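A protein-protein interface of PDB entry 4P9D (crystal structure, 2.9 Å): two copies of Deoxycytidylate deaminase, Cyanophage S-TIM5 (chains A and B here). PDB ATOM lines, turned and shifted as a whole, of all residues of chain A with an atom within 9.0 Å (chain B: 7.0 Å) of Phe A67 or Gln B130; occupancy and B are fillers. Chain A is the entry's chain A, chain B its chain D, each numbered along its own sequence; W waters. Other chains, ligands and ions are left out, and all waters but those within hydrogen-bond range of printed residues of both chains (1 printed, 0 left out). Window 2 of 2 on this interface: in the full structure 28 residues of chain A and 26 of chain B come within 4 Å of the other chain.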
ATOM      1  N   CYS A  25      17.684  -6.798 -18.690  1.00  0.00           N
ATOM      2  CA  CYS A  25      16.445  -6.109 -18.346  1.00  0.00           C
ATOM      3  C   CYS A  25      16.698  -4.640 -18.029  1.00  0.00           C
ATOM      4  O   CYS A  25      17.699  -4.298 -17.403  1.00  0.00           O
ATOM      5  CB  CYS A  25      15.761  -6.795 -17.161  1.00  0.00           C
ATOM      6  SG  CYS A  25      15.443  -8.559 -17.399  1.00  0.00           S
ATOM      7  N   ASN A  46      18.466 -11.527 -13.095  1.00  0.00           N
ATOM      8  CA  ASN A  46      17.191 -11.668 -13.784  1.00  0.00           C
ATOM      9  C   ASN A  46      17.343 -11.684 -15.300  1.00  0.00           C
ATOM     10  O   ASN A  46      18.180 -10.979 -15.861  1.00  0.00           O
ATOM     11  CB  ASN A  46      16.234 -10.551 -13.370  1.00  0.00           C
ATOM     12  CG  ASN A  46      16.801  -9.172 -13.630  1.00  0.00           C
ATOM     13  OD1 ASN A  46      18.011  -8.960 -13.548  1.00  0.00           O
ATOM     14  ND2 ASN A  46      15.927  -8.223 -13.944  1.00  0.00           N
ATOM     15  N   GLY A  47      16.521 -12.499 -15.953  1.00  0.00           N
ATOM     16  CA  GLY A  47      16.541 -12.608 -17.400  1.00  0.00           C
ATOM     17  C   GLY A  47      15.708 -13.772 -17.900  1.00  0.00           C
ATOM     18  O   GLY A  47      15.072 -14.477 -17.117  1.00  0.00           O
ATOM     19  N   THR A  48      15.716 -13.970 -19.214  1.00  0.00           N
ATOM     20  CA  THR A  48      14.978 -15.060 -19.838  1.00  0.00           C
ATOM     21  C   THR A  48      15.664 -16.395 -19.557  1.00  0.00           C
ATOM     22  O   THR A  48      16.848 -16.417 -19.226  1.00  0.00           O
ATOM     23  CB  THR A  48      14.858 -14.848 -21.360  1.00  0.00           C
ATOM     24  OG1 THR A  48      16.152 -14.961 -21.965  1.00  0.00           O
ATOM     25  CG2 THR A  48      14.275 -13.477 -21.662  1.00  0.00           C
ATOM     26  N   PRO A  49      14.925 -17.512 -19.672  1.00  0.00           N
ATOM     27  CA  PRO A  49      15.545 -18.832 -19.499  1.00  0.00           C
ATOM     28  C   PRO A  49      16.707 -19.077 -20.462  1.00  0.00           C
ATOM     29  O   PRO A  49      16.855 -18.356 -21.448  1.00  0.00           O
ATOM     30  CB  PRO A  49      14.394 -19.799 -19.786  1.00  0.00           C
ATOM     31  CG  PRO A  49      13.171 -19.034 -19.437  1.00  0.00           C
ATOM     32  CD  PRO A  49      13.460 -17.609 -19.815  1.00  0.00           C
ATOM     33  N   SER A  50      17.525 -20.083 -20.167  1.00  0.00           N
ATOM     34  CA  SER A  50      18.661 -20.414 -21.016  1.00  0.00           C
ATOM     35  C   SER A  50      18.202 -20.866 -22.397  1.00  0.00           C
ATOM     36  O   SER A  50      17.315 -21.711 -22.522  1.00  0.00           O
ATOM     37  CB  SER A  50      19.520 -21.502 -20.369  1.00  0.00           C
ATOM     38  OG  SER A  50      19.884 -21.146 -19.046  1.00  0.00           O
ATOM     39  N   GLY A  51      18.806 -20.292 -23.431  1.00  0.00           N
ATOM     40  CA  GLY A  51      18.491 -20.660 -24.797  1.00  0.00           C
ATOM     41  C   GLY A  51      17.219 -20.028 -25.323  1.00  0.00           C
ATOM     42  O   GLY A  51      16.758 -20.366 -26.414  1.00  0.00           O
ATOM     43  N   PHE A  52      16.647 -19.114 -24.547  1.00  0.00           N
ATOM     44  CA  PHE A  52      15.450 -18.400 -24.972  1.00  0.00           C
ATOM     45  C   PHE A  52      15.788 -17.547 -26.189  1.00  0.00           C
ATOM     46  O   PHE A  52      16.917 -17.078 -26.324  1.00  0.00           O
ATOM     47  CB  PHE A  52      14.902 -17.540 -23.834  1.00  0.00           C
ATOM     48  CG  PHE A  52      13.447 -17.205 -23.973  1.00  0.00           C
ATOM     49  CD1 PHE A  52      12.483 -18.191 -23.858  1.00  0.00           C
ATOM     50  CD2 PHE A  52      13.042 -15.901 -24.203  1.00  0.00           C
ATOM     51  CE1 PHE A  52      11.143 -17.887 -23.980  1.00  0.00           C
ATOM     52  CE2 PHE A  52      11.703 -15.590 -24.323  1.00  0.00           C
ATOM     53  CZ  PHE A  52      10.752 -16.585 -24.213  1.00  0.00           C
ATOM     54  N   HIS A  53      14.813 -17.357 -27.073  1.00  0.00           N
ATOM     55  CA  HIS A  53      15.052 -16.711 -28.364  1.00  0.00           C
ATOM     56  C   HIS A  53      15.634 -15.303 -28.242  1.00  0.00           C
ATOM     57  O   HIS A  53      16.461 -14.899 -29.059  1.00  0.00           O
ATOM     58  CB  HIS A  53      13.758 -16.664 -29.178  1.00  0.00           C
ATOM     59  CG  HIS A  53      12.614 -16.015 -28.465  1.00  0.00           C
ATOM     60  ND1 HIS A  53      12.445 -14.645 -28.416  1.00  0.00           N
ATOM     61  CD2 HIS A  53      11.572 -16.543 -27.785  1.00  0.00           C
ATOM     62  CE1 HIS A  53      11.353 -14.362 -27.735  1.00  0.00           C
ATOM     63  NE2 HIS A  53      10.801 -15.500 -27.338  1.00  0.00           N
ATOM     64  N   THR A  54      15.205 -14.561 -27.227  1.00  0.00           N
ATOM     65  CA  THR A  54      15.759 -13.234 -26.985  1.00  0.00           C
ATOM     66  C   THR A  54      16.269 -13.117 -25.554  1.00  0.00           C
ATOM     67  O   THR A  54      15.747 -13.759 -24.641  1.00  0.00           O
ATOM     68  CB  THR A  54      14.723 -12.120 -27.251  1.00  0.00           C
ATOM     69  OG1 THR A  54      15.346 -10.839 -27.091  1.00  0.00           O
ATOM     70  CG2 THR A  54      13.552 -12.226 -26.286  1.00  0.00           C
ATOM     71  N   CYS A  56      16.397 -10.094 -24.308  1.00  0.00           N
ATOM     72  CA  CYS A  56      15.638  -8.930 -23.873  1.00  0.00           C
ATOM     73  C   CYS A  56      14.522  -9.384 -22.941  1.00  0.00           C
ATOM     74  O   CYS A  56      13.846 -10.375 -23.214  1.00  0.00           O
ATOM     75  CB  CYS A  56      15.065  -8.173 -25.072  1.00  0.00           C
ATOM     76  SG  CYS A  56      13.689  -7.071 -24.674  1.00  0.00           S
ATOM     77  N   CYS A  57      14.333  -8.663 -21.842  1.00  0.00           N
ATOM     78  CA  CYS A  57      13.368  -9.077 -20.827  1.00  0.00           C
ATOM     79  C   CYS A  57      12.033  -8.348 -20.938  1.00  0.00           C
ATOM     80  O   CYS A  57      11.065  -8.714 -20.276  1.00  0.00           O
ATOM     81  CB  CYS A  57      13.957  -8.869 -19.428  1.00  0.00           C
ATOM     82  SG  CYS A  57      15.731  -9.191 -19.308  1.00  0.00           S
ATOM     83  N   LEU A  59       8.594  -6.642 -22.878  1.00  0.00           N
ATOM     84  CA  LEU A  59       7.624  -6.807 -23.951  1.00  0.00           C
ATOM     85  C   LEU A  59       7.663  -5.592 -24.867  1.00  0.00           C
ATOM     86  O   LEU A  59       8.399  -4.639 -24.613  1.00  0.00           O
ATOM     87  CB  LEU A  59       6.216  -6.992 -23.380  1.00  0.00           C
ATOM     88  CG  LEU A  59       5.913  -8.222 -22.526  1.00  0.00           C
ATOM     89  CD1 LEU A  59       4.533  -8.087 -21.907  1.00  0.00           C
ATOM     90  CD2 LEU A  59       6.000  -9.490 -23.359  1.00  0.00           C
ATOM     91  N   SER A  63       6.688  -3.747 -20.528  1.00  0.00           N
ATOM     92  CA  SER A  63       6.328  -4.648 -19.439  1.00  0.00           C
ATOM     93  C   SER A  63       7.283  -5.830 -19.355  1.00  0.00           C
ATOM     94  O   SER A  63       8.092  -6.053 -20.254  1.00  0.00           O
ATOM     95  CB  SER A  63       4.892  -5.148 -19.602  1.00  0.00           C
ATOM     96  OG  SER A  63       4.628  -6.223 -18.716  1.00  0.00           O
ATOM     97  N   THR A  64       7.181  -6.588 -18.269  1.00  0.00           N
ATOM     98  CA  THR A  64       8.060  -7.726 -18.046  1.00  0.00           C
ATOM     99  C   THR A  64       7.465  -9.017 -18.603  1.00  0.00           C
ATOM    100  O   THR A  64       6.351  -9.406 -18.248  1.00  0.00           O
ATOM    101  CB  THR A  64       8.365  -7.904 -16.543  1.00  0.00           C
ATOM    102  OG1 THR A  64       9.394  -6.986 -16.154  1.00  0.00           O
ATOM    103  CG2 THR A  64       8.835  -9.314 -16.253  1.00  0.00           C
ATOM    104  N   ASN A  65       8.215  -9.658 -19.495  1.00  0.00           N
ATOM    105  CA  ASN A  65       7.863 -10.972 -20.020  1.00  0.00           C
ATOM    106  C   ASN A  65       7.672 -11.947 -18.865  1.00  0.00           C
ATOM    107  O   ASN A  65       8.579 -12.138 -18.059  1.00  0.00           O
ATOM    108  CB  ASN A  65       8.955 -11.462 -20.982  1.00  0.00           C
ATOM    109  CG  ASN A  65       8.559 -12.714 -21.756  1.00  0.00           C
ATOM    110  OD1 ASN A  65       7.633 -13.432 -21.386  1.00  0.00           O
ATOM    111  ND2 ASN A  65       9.277 -12.979 -22.842  1.00  0.00           N
ATOM    112  N   PRO A  66       6.483 -12.566 -18.772  1.00  0.00           N
ATOM    113  CA  PRO A  66       6.209 -13.523 -17.692  1.00  0.00           C
ATOM    114  C   PRO A  66       7.125 -14.749 -17.721  1.00  0.00           C
ATOM    115  O   PRO A  66       7.043 -15.593 -16.828  1.00  0.00           O
ATOM    116  CB  PRO A  66       4.749 -13.925 -17.942  1.00  0.00           C
ATOM    117  CG  PRO A  66       4.507 -13.613 -19.384  1.00  0.00           C
ATOM    118  CD  PRO A  66       5.314 -12.380 -19.648  1.00  0.00           C
ATOM    119  N   PHE A  67       7.986 -14.836 -18.729  1.00  0.00           N
ATOM    120  CA  PHE A  67       8.936 -15.935 -18.845  1.00  0.00           C
ATOM    121  C   PHE A  67      10.238 -15.679 -18.092  1.00  0.00           C
ATOM    122  O   PHE A  67      10.994 -16.612 -17.826  1.00  0.00           O
ATOM    123  CB  PHE A  67       9.250 -16.212 -20.316  1.00  0.00           C
ATOM    124  CG  PHE A  67       8.307 -17.181 -20.965  1.00  0.00           C
ATOM    125  CD1 PHE A  67       8.374 -18.532 -20.670  1.00  0.00           C
ATOM    126  CD2 PHE A  67       7.356 -16.744 -21.872  1.00  0.00           C
ATOM    127  CE1 PHE A  67       7.510 -19.429 -21.264  1.00  0.00           C
ATOM    128  CE2 PHE A  67       6.488 -17.637 -22.470  1.00  0.00           C
ATOM    129  CZ  PHE A  67       6.565 -18.982 -22.166  1.00  0.00           C
ATOM    130  N   VAL A  68      10.505 -14.420 -17.753  1.00  0.00           N
ATOM    131  CA  VAL A  68      11.772 -14.077 -17.114  1.00  0.00           C
ATOM    132  C   VAL A  68      11.877 -14.695 -15.726  1.00  0.00           C
ATOM    133  O   VAL A  68      10.871 -14.985 -15.078  1.00  0.00           O
ATOM    134  CB  VAL A  68      11.976 -12.551 -16.992  1.00  0.00           C
ATOM    135  CG1 VAL A  68      11.717 -11.866 -18.326  1.00  0.00           C
ATOM    136  CG2 VAL A  68      11.092 -11.975 -15.900  1.00  0.00           C
ATOM    137  N   LEU A  69      13.111 -14.904 -15.287  1.00  0.00           N
ATOM    138  CA  LEU A  69      13.378 -15.458 -13.971  1.00  0.00           C
ATOM    139  C   LEU A  69      13.885 -14.361 -13.049  1.00  0.00           C
ATOM    140  O   LEU A  69      14.610 -13.469 -13.483  1.00  0.00           O
ATOM    141  CB  LEU A  69      14.404 -16.589 -14.063  1.00  0.00           C
ATOM    142  CG  LEU A  69      13.995 -17.834 -14.853  1.00  0.00           C
ATOM    143  CD1 LEU A  69      15.178 -18.378 -15.633  1.00  0.00           C
ATOM    144  CD2 LEU A  69      13.439 -18.899 -13.920  1.00  0.00           C
ATOM    145  N   HIS A  70      13.493 -14.415 -11.782  1.00  0.00           N
ATOM    146  CA  HIS A  70      14.056 -13.504 -10.797  1.00  0.00           C
ATOM    147  C   HIS A  70      15.495 -13.912 -10.510  1.00  0.00           C
ATOM    148  O   HIS A  70      15.865 -15.072 -10.697  1.00  0.00           O
ATOM    149  CB  HIS A  70      13.226 -13.499  -9.511  1.00  0.00           C
ATOM    150  CG  HIS A  70      11.936 -12.758  -9.628  1.00  0.00           C
ATOM    151  ND1 HIS A  70      11.072 -12.583  -8.565  1.00  0.00           N
ATOM    152  CD2 HIS A  70      11.351 -12.134 -10.685  1.00  0.00           C
ATOM    153  CE1 HIS A  70      10.020 -11.891  -8.963  1.00  0.00           C
ATOM    154  NE2 HIS A  70      10.165 -11.608 -10.239  1.00  0.00           N
ATOM    155  N   GLN A  73      15.524 -16.591  -8.172  1.00  0.00           N
ATOM    156  CA  GLN A  73      15.072 -17.838  -8.780  1.00  0.00           C
ATOM    157  C   GLN A  73      16.220 -18.554  -9.480  1.00  0.00           C
ATOM    158  O   GLN A  73      16.410 -19.759  -9.305  1.00  0.00           O
ATOM    159  CB  GLN A  73      13.938 -17.575  -9.772  1.00  0.00           C
ATOM    160  CG  GLN A  73      12.547 -17.776  -9.198  1.00  0.00           C
ATOM    161  CD  GLN A  73      11.455 -17.423 -10.188  1.00  0.00           C
ATOM    162  OE1 GLN A  73      11.580 -16.463 -10.950  1.00  0.00           O
ATOM    163  NE2 GLN A  73      10.380 -18.201 -10.187  1.00  0.00           N
ATOM    164  N   ASN A  74      16.980 -17.807 -10.274  1.00  0.00           N
ATOM    165  CA  ASN A  74      18.141 -18.355 -10.966  1.00  0.00           C
ATOM    166  C   ASN A  74      19.214 -18.813  -9.988  1.00  0.00           C
ATOM    167  O   ASN A  74      19.904 -19.800 -10.232  1.00  0.00           O
ATOM    168  CB  ASN A  74      18.727 -17.327 -11.932  1.00  0.00           C
ATOM    169  CG  ASN A  74      18.109 -17.406 -13.311  1.00  0.00           C
ATOM    170  OD1 ASN A  74      17.912 -18.493 -13.855  1.00  0.00           O
ATOM    171  ND2 ASN A  74      17.804 -16.250 -13.891  1.00  0.00           N
ATOM    172  N   PRO B  99       2.829 -22.469 -14.581  1.00  0.00           N
ATOM    173  CA  PRO B  99       3.767 -21.696 -15.404  1.00  0.00           C
ATOM    174  C   PRO B  99       5.037 -21.265 -14.668  1.00  0.00           C
ATOM    175  O   PRO B  99       6.121 -21.334 -15.244  1.00  0.00           O
ATOM    176  CB  PRO B  99       2.940 -20.473 -15.803  1.00  0.00           C
ATOM    177  CG  PRO B  99       1.553 -20.993 -15.880  1.00  0.00           C
ATOM    178  CD  PRO B  99       1.435 -22.031 -14.792  1.00  0.00           C
ATOM    179  N   LYS B 103       8.689 -22.794 -15.539  1.00  0.00           N
ATOM    180  CA  LYS B 103       9.757 -21.850 -15.843  1.00  0.00           C
ATOM    181  C   LYS B 103      11.061 -22.249 -15.162  1.00  0.00           C
ATOM    182  O   LYS B 103      12.129 -22.231 -15.775  1.00  0.00           O
ATOM    183  CB  LYS B 103       9.346 -20.446 -15.404  1.00  0.00           C
ATOM    184  CG  LYS B 103      10.286 -19.338 -15.833  1.00  0.00           C
ATOM    185  CD  LYS B 103      10.059 -18.101 -14.981  1.00  0.00           C
ATOM    186  CE  LYS B 103       8.581 -17.755 -14.896  1.00  0.00           C
ATOM    187  NZ  LYS B 103       8.323 -16.630 -13.956  1.00  0.00           N
ATOM    188  N   ASP B 123      -1.456 -24.010 -18.941  1.00  0.00           N
ATOM    189  CA  ASP B 123      -0.391 -23.179 -19.493  1.00  0.00           C
ATOM    190  C   ASP B 123       0.998 -23.659 -19.071  1.00  0.00           C
ATOM    191  O   ASP B 123       1.982 -23.396 -19.759  1.00  0.00           O
ATOM    192  CB  ASP B 123      -0.599 -21.720 -19.089  1.00  0.00           C
ATOM    193  CG  ASP B 123      -1.921 -21.170 -19.583  1.00  0.00           C
ATOM    194  OD1 ASP B 123      -2.468 -21.733 -20.556  1.00  0.00           O
ATOM    195  OD2 ASP B 123      -2.414 -20.176 -19.011  1.00  0.00           O
ATOM    196  N   ILE B 125       2.132 -26.751 -19.028  1.00  0.00           N
ATOM    197  CA  ILE B 125       2.585 -27.658 -20.076  1.00  0.00           C
ATOM    198  C   ILE B 125       3.153 -26.854 -21.237  1.00  0.00           C
ATOM    199  O   ILE B 125       4.254 -27.124 -21.709  1.00  0.00           O
ATOM    200  CB  ILE B 125       1.446 -28.560 -20.594  1.00  0.00           C
ATOM    201  CG1 ILE B 125       0.738 -29.264 -19.435  1.00  0.00           C
ATOM    202  CG2 ILE B 125       1.980 -29.573 -21.597  1.00  0.00           C
ATOM    203  CD1 ILE B 125      -0.512 -30.010 -19.855  1.00  0.00           C
ATOM    204  N   ASP B 126       2.390 -25.854 -21.674  1.00  0.00           N
ATOM    205  CA  ASP B 126       2.781 -24.972 -22.770  1.00  0.00           C
ATOM    206  C   ASP B 126       4.137 -24.311 -22.528  1.00  0.00           C
ATOM    207  O   ASP B 126       4.935 -24.158 -23.453  1.00  0.00           O
ATOM    208  CB  ASP B 126       1.707 -23.902 -22.989  1.00  0.00           C
ATOM    209  CG  ASP B 126       2.037 -22.961 -24.133  1.00  0.00           C
ATOM    210  OD1 ASP B 126       2.089 -23.421 -25.292  1.00  0.00           O
ATOM    211  OD2 ASP B 126       2.240 -21.756 -23.870  1.00  0.00           O
ATOM    212  N   VAL B 127       4.393 -23.921 -21.282  1.00  0.00           N
ATOM    213  CA  VAL B 127       5.667 -23.309 -20.921  1.00  0.00           C
ATOM    214  C   VAL B 127       6.807 -24.316 -21.063  1.00  0.00           C
ATOM    215  O   VAL B 127       7.896 -23.976 -21.528  1.00  0.00           O
ATOM    216  CB  VAL B 127       5.639 -22.750 -19.481  1.00  0.00           C
ATOM    217  CG1 VAL B 127       7.022 -22.274 -19.058  1.00  0.00           C
ATOM    218  CG2 VAL B 127       4.634 -21.616 -19.374  1.00  0.00           C
ATOM    219  N   LEU B 128       6.543 -25.560 -20.674  1.00  0.00           N
ATOM    220  CA  LEU B 128       7.542 -26.621 -20.751  1.00  0.00           C
ATOM    221  C   LEU B 128       7.953 -26.928 -22.190  1.00  0.00           C
ATOM    222  O   LEU B 128       9.144 -27.016 -22.493  1.00  0.00           O
ATOM    223  CB  LEU B 128       7.021 -27.893 -20.082  1.00  0.00           C
ATOM    224  CG  LEU B 128       6.888 -27.848 -18.560  1.00  0.00           C
ATOM    225  CD1 LEU B 128       6.266 -29.135 -18.044  1.00  0.00           C
ATOM    226  CD2 LEU B 128       8.247 -27.613 -17.923  1.00  0.00           C
ATOM    227  N   GLN B 129       6.968 -27.099 -23.068  1.00  0.00           N
ATOM    228  CA  GLN B 129       7.236 -27.387 -24.475  1.00  0.00           C
ATOM    229  C   GLN B 129       8.022 -26.250 -25.115  1.00  0.00           C
ATOM    230  O   GLN B 129       8.978 -26.479 -25.857  1.00  0.00           O
ATOM    231  CB  GLN B 129       5.933 -27.612 -25.246  1.00  0.00           C
ATOM    232  CG  GLN B 129       4.837 -28.302 -24.454  1.00  0.00           C
ATOM    233  CD  GLN B 129       4.450 -29.650 -25.027  1.00  0.00           C
ATOM    234  OE1 GLN B 129       5.307 -30.480 -25.330  1.00  0.00           O
ATOM    235  NE2 GLN B 129       3.150 -29.874 -25.180  1.00  0.00           N
ATOM    236  N   GLN B 130       7.599 -25.025 -24.818  1.00  0.00           N
ATOM    237  CA  GLN B 130       8.238 -23.820 -25.334  1.00  0.00           C
ATOM    238  C   GLN B 130       9.722 -23.772 -24.989  1.00  0.00           C
ATOM    239  O   GLN B 130      10.549 -23.382 -25.813  1.00  0.00           O
ATOM    240  CB  GLN B 130       7.531 -22.578 -24.782  1.00  0.00           C
ATOM    241  CG  GLN B 130       8.333 -21.292 -24.889  1.00  0.00           C
ATOM    242  CD  GLN B 130       8.277 -20.684 -26.274  1.00  0.00           C
ATOM    243  OE1 GLN B 130       7.216 -20.624 -26.895  1.00  0.00           O
ATOM    244  NE2 GLN B 130       9.423 -20.229 -26.767  1.00  0.00           N
ATOM    245  N   LEU B 131      10.054 -24.182 -23.770  1.00  0.00           N
ATOM    246  CA  LEU B 131      11.431 -24.133 -23.297  1.00  0.00           C
ATOM    247  C   LEU B 131      12.168 -25.448 -23.542  1.00  0.00           C
ATOM    248  O   LEU B 131      13.212 -25.707 -22.943  1.00  0.00           O
ATOM    249  CB  LEU B 131      11.465 -23.775 -21.811  1.00  0.00           C
ATOM    250  CG  LEU B 131      10.894 -22.397 -21.468  1.00  0.00           C
ATOM    251  CD1 LEU B 131      10.814 -22.193 -19.965  1.00  0.00           C
ATOM    252  CD2 LEU B 131      11.730 -21.303 -22.116  1.00  0.00           C
ATOM    253  N   GLY B 132      11.615 -26.277 -24.423  1.00  0.00           N
ATOM    254  CA  GLY B 132      12.287 -27.485 -24.866  1.00  0.00           C
ATOM    255  C   GLY B 132      12.338 -28.620 -23.861  1.00  0.00           C
ATOM    256  O   GLY B 132      13.303 -29.382 -23.831  1.00  0.00           O
ATOM    257  N   VAL B 133      11.302 -28.737 -23.037  1.00  0.00           N
ATOM    258  CA  VAL B 133      11.205 -29.848 -22.096  1.00  0.00           C
ATOM    259  C   VAL B 133      10.211 -30.884 -22.607  1.00  0.00           C
ATOM    260  O   VAL B 133       9.046 -30.566 -22.847  1.00  0.00           O
ATOM    261  CB  VAL B 133      10.773 -29.376 -20.694  1.00  0.00           C
ATOM    262  CG1 VAL B 133      10.422 -30.569 -19.814  1.00  0.00           C
ATOM    263  CG2 VAL B 133      11.865 -28.533 -20.054  1.00  0.00           C
HETATM  264  O   HOH W   1       5.394 -16.832 -14.497  1.00  0.00           O
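Of the printed residues of chain B, Phe A67 touches Lys B103, Val B127 and Gln B130. Of the printed residues of chain A, Gln B130 touches Phe A67. Of chain A, only Pro A49 and Phe A52 come within 4 Å of Leu B131. Of the printed residues of chain A, Lys B103 touches Pro A66 (3.3 Å), Phe A67 (3.3 Å), Val A68 (3.2 Å) and Leu A69 (3.6 Å). Printed residues of chain B within 4 Å of Pro A66: Lys B103 (3.3 Å). Printed residues of chain B within 4 Å of Phe A52: Leu B131. Printed residues of chain B within 4 Å of Leu A69: Lys B103. Of the printed residues of chain B, Pro A49 touches Leu B131 (3.8 Å). Cys A57 touches none of the printed residues of chain B. Cys A56 touches none of the printed residues of chain B.
Pro A49 touches Leu B131. CD2 of Leu B131 touches CD1 of Phe A52, at 3.6 Å. Lys B103 touches Phe A67. CE1 of Phe A67 touches CG1 of Val B127, at 3.6 Å. Gln B130 touches Phe A67. CD of Lys B103 touches CD2 of Leu A69, 3.6 Å away.
O of Pro A66 lies close to NZ of Lys B103, at 3.3 Å. O of Val A68 sits close to NZ of Lys B103 (3.2 Å).
Of the 12 printed residues of chain B, 4 touch a printed residue of chain A. Along chain B the printed residues that touch a printed residue of chain A span positions 103 to 131. Printed residues of chain A that touch a printed residue of chain B: Pro A49, Phe A52, Pro A66, Phe A67, Val A68 and Leu A69. Hydrophobic or aromatic side chains of chain A that line the printed part of chain B: Pro A49, Phe A52, Phe A67 and Leu A69. Among the printed residues, 8 pairs touch across the chains. Among the printed residues, no Asp or Glu carboxylate lies within 4 Å of a Lys or Arg side-chain nitrogen of the other chain.
Water W1 bridges NZ of Lys B103 (3.0 Å) and O of Pro A66 (3.1 Å).
The side-chain sulfur (SG) of Cys A25 forms a disulfide with the side-chain sulfur (SG) of Cys A57. OD1 of Asn A65 sits close to N of Phe A67 (3.0 Å). The backbone carbonyl oxygen of Gly A47 sits at hydrogen-bond distance from the backbone NH of Leu A69 (2.7 Å).
No position is printed for both chains.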
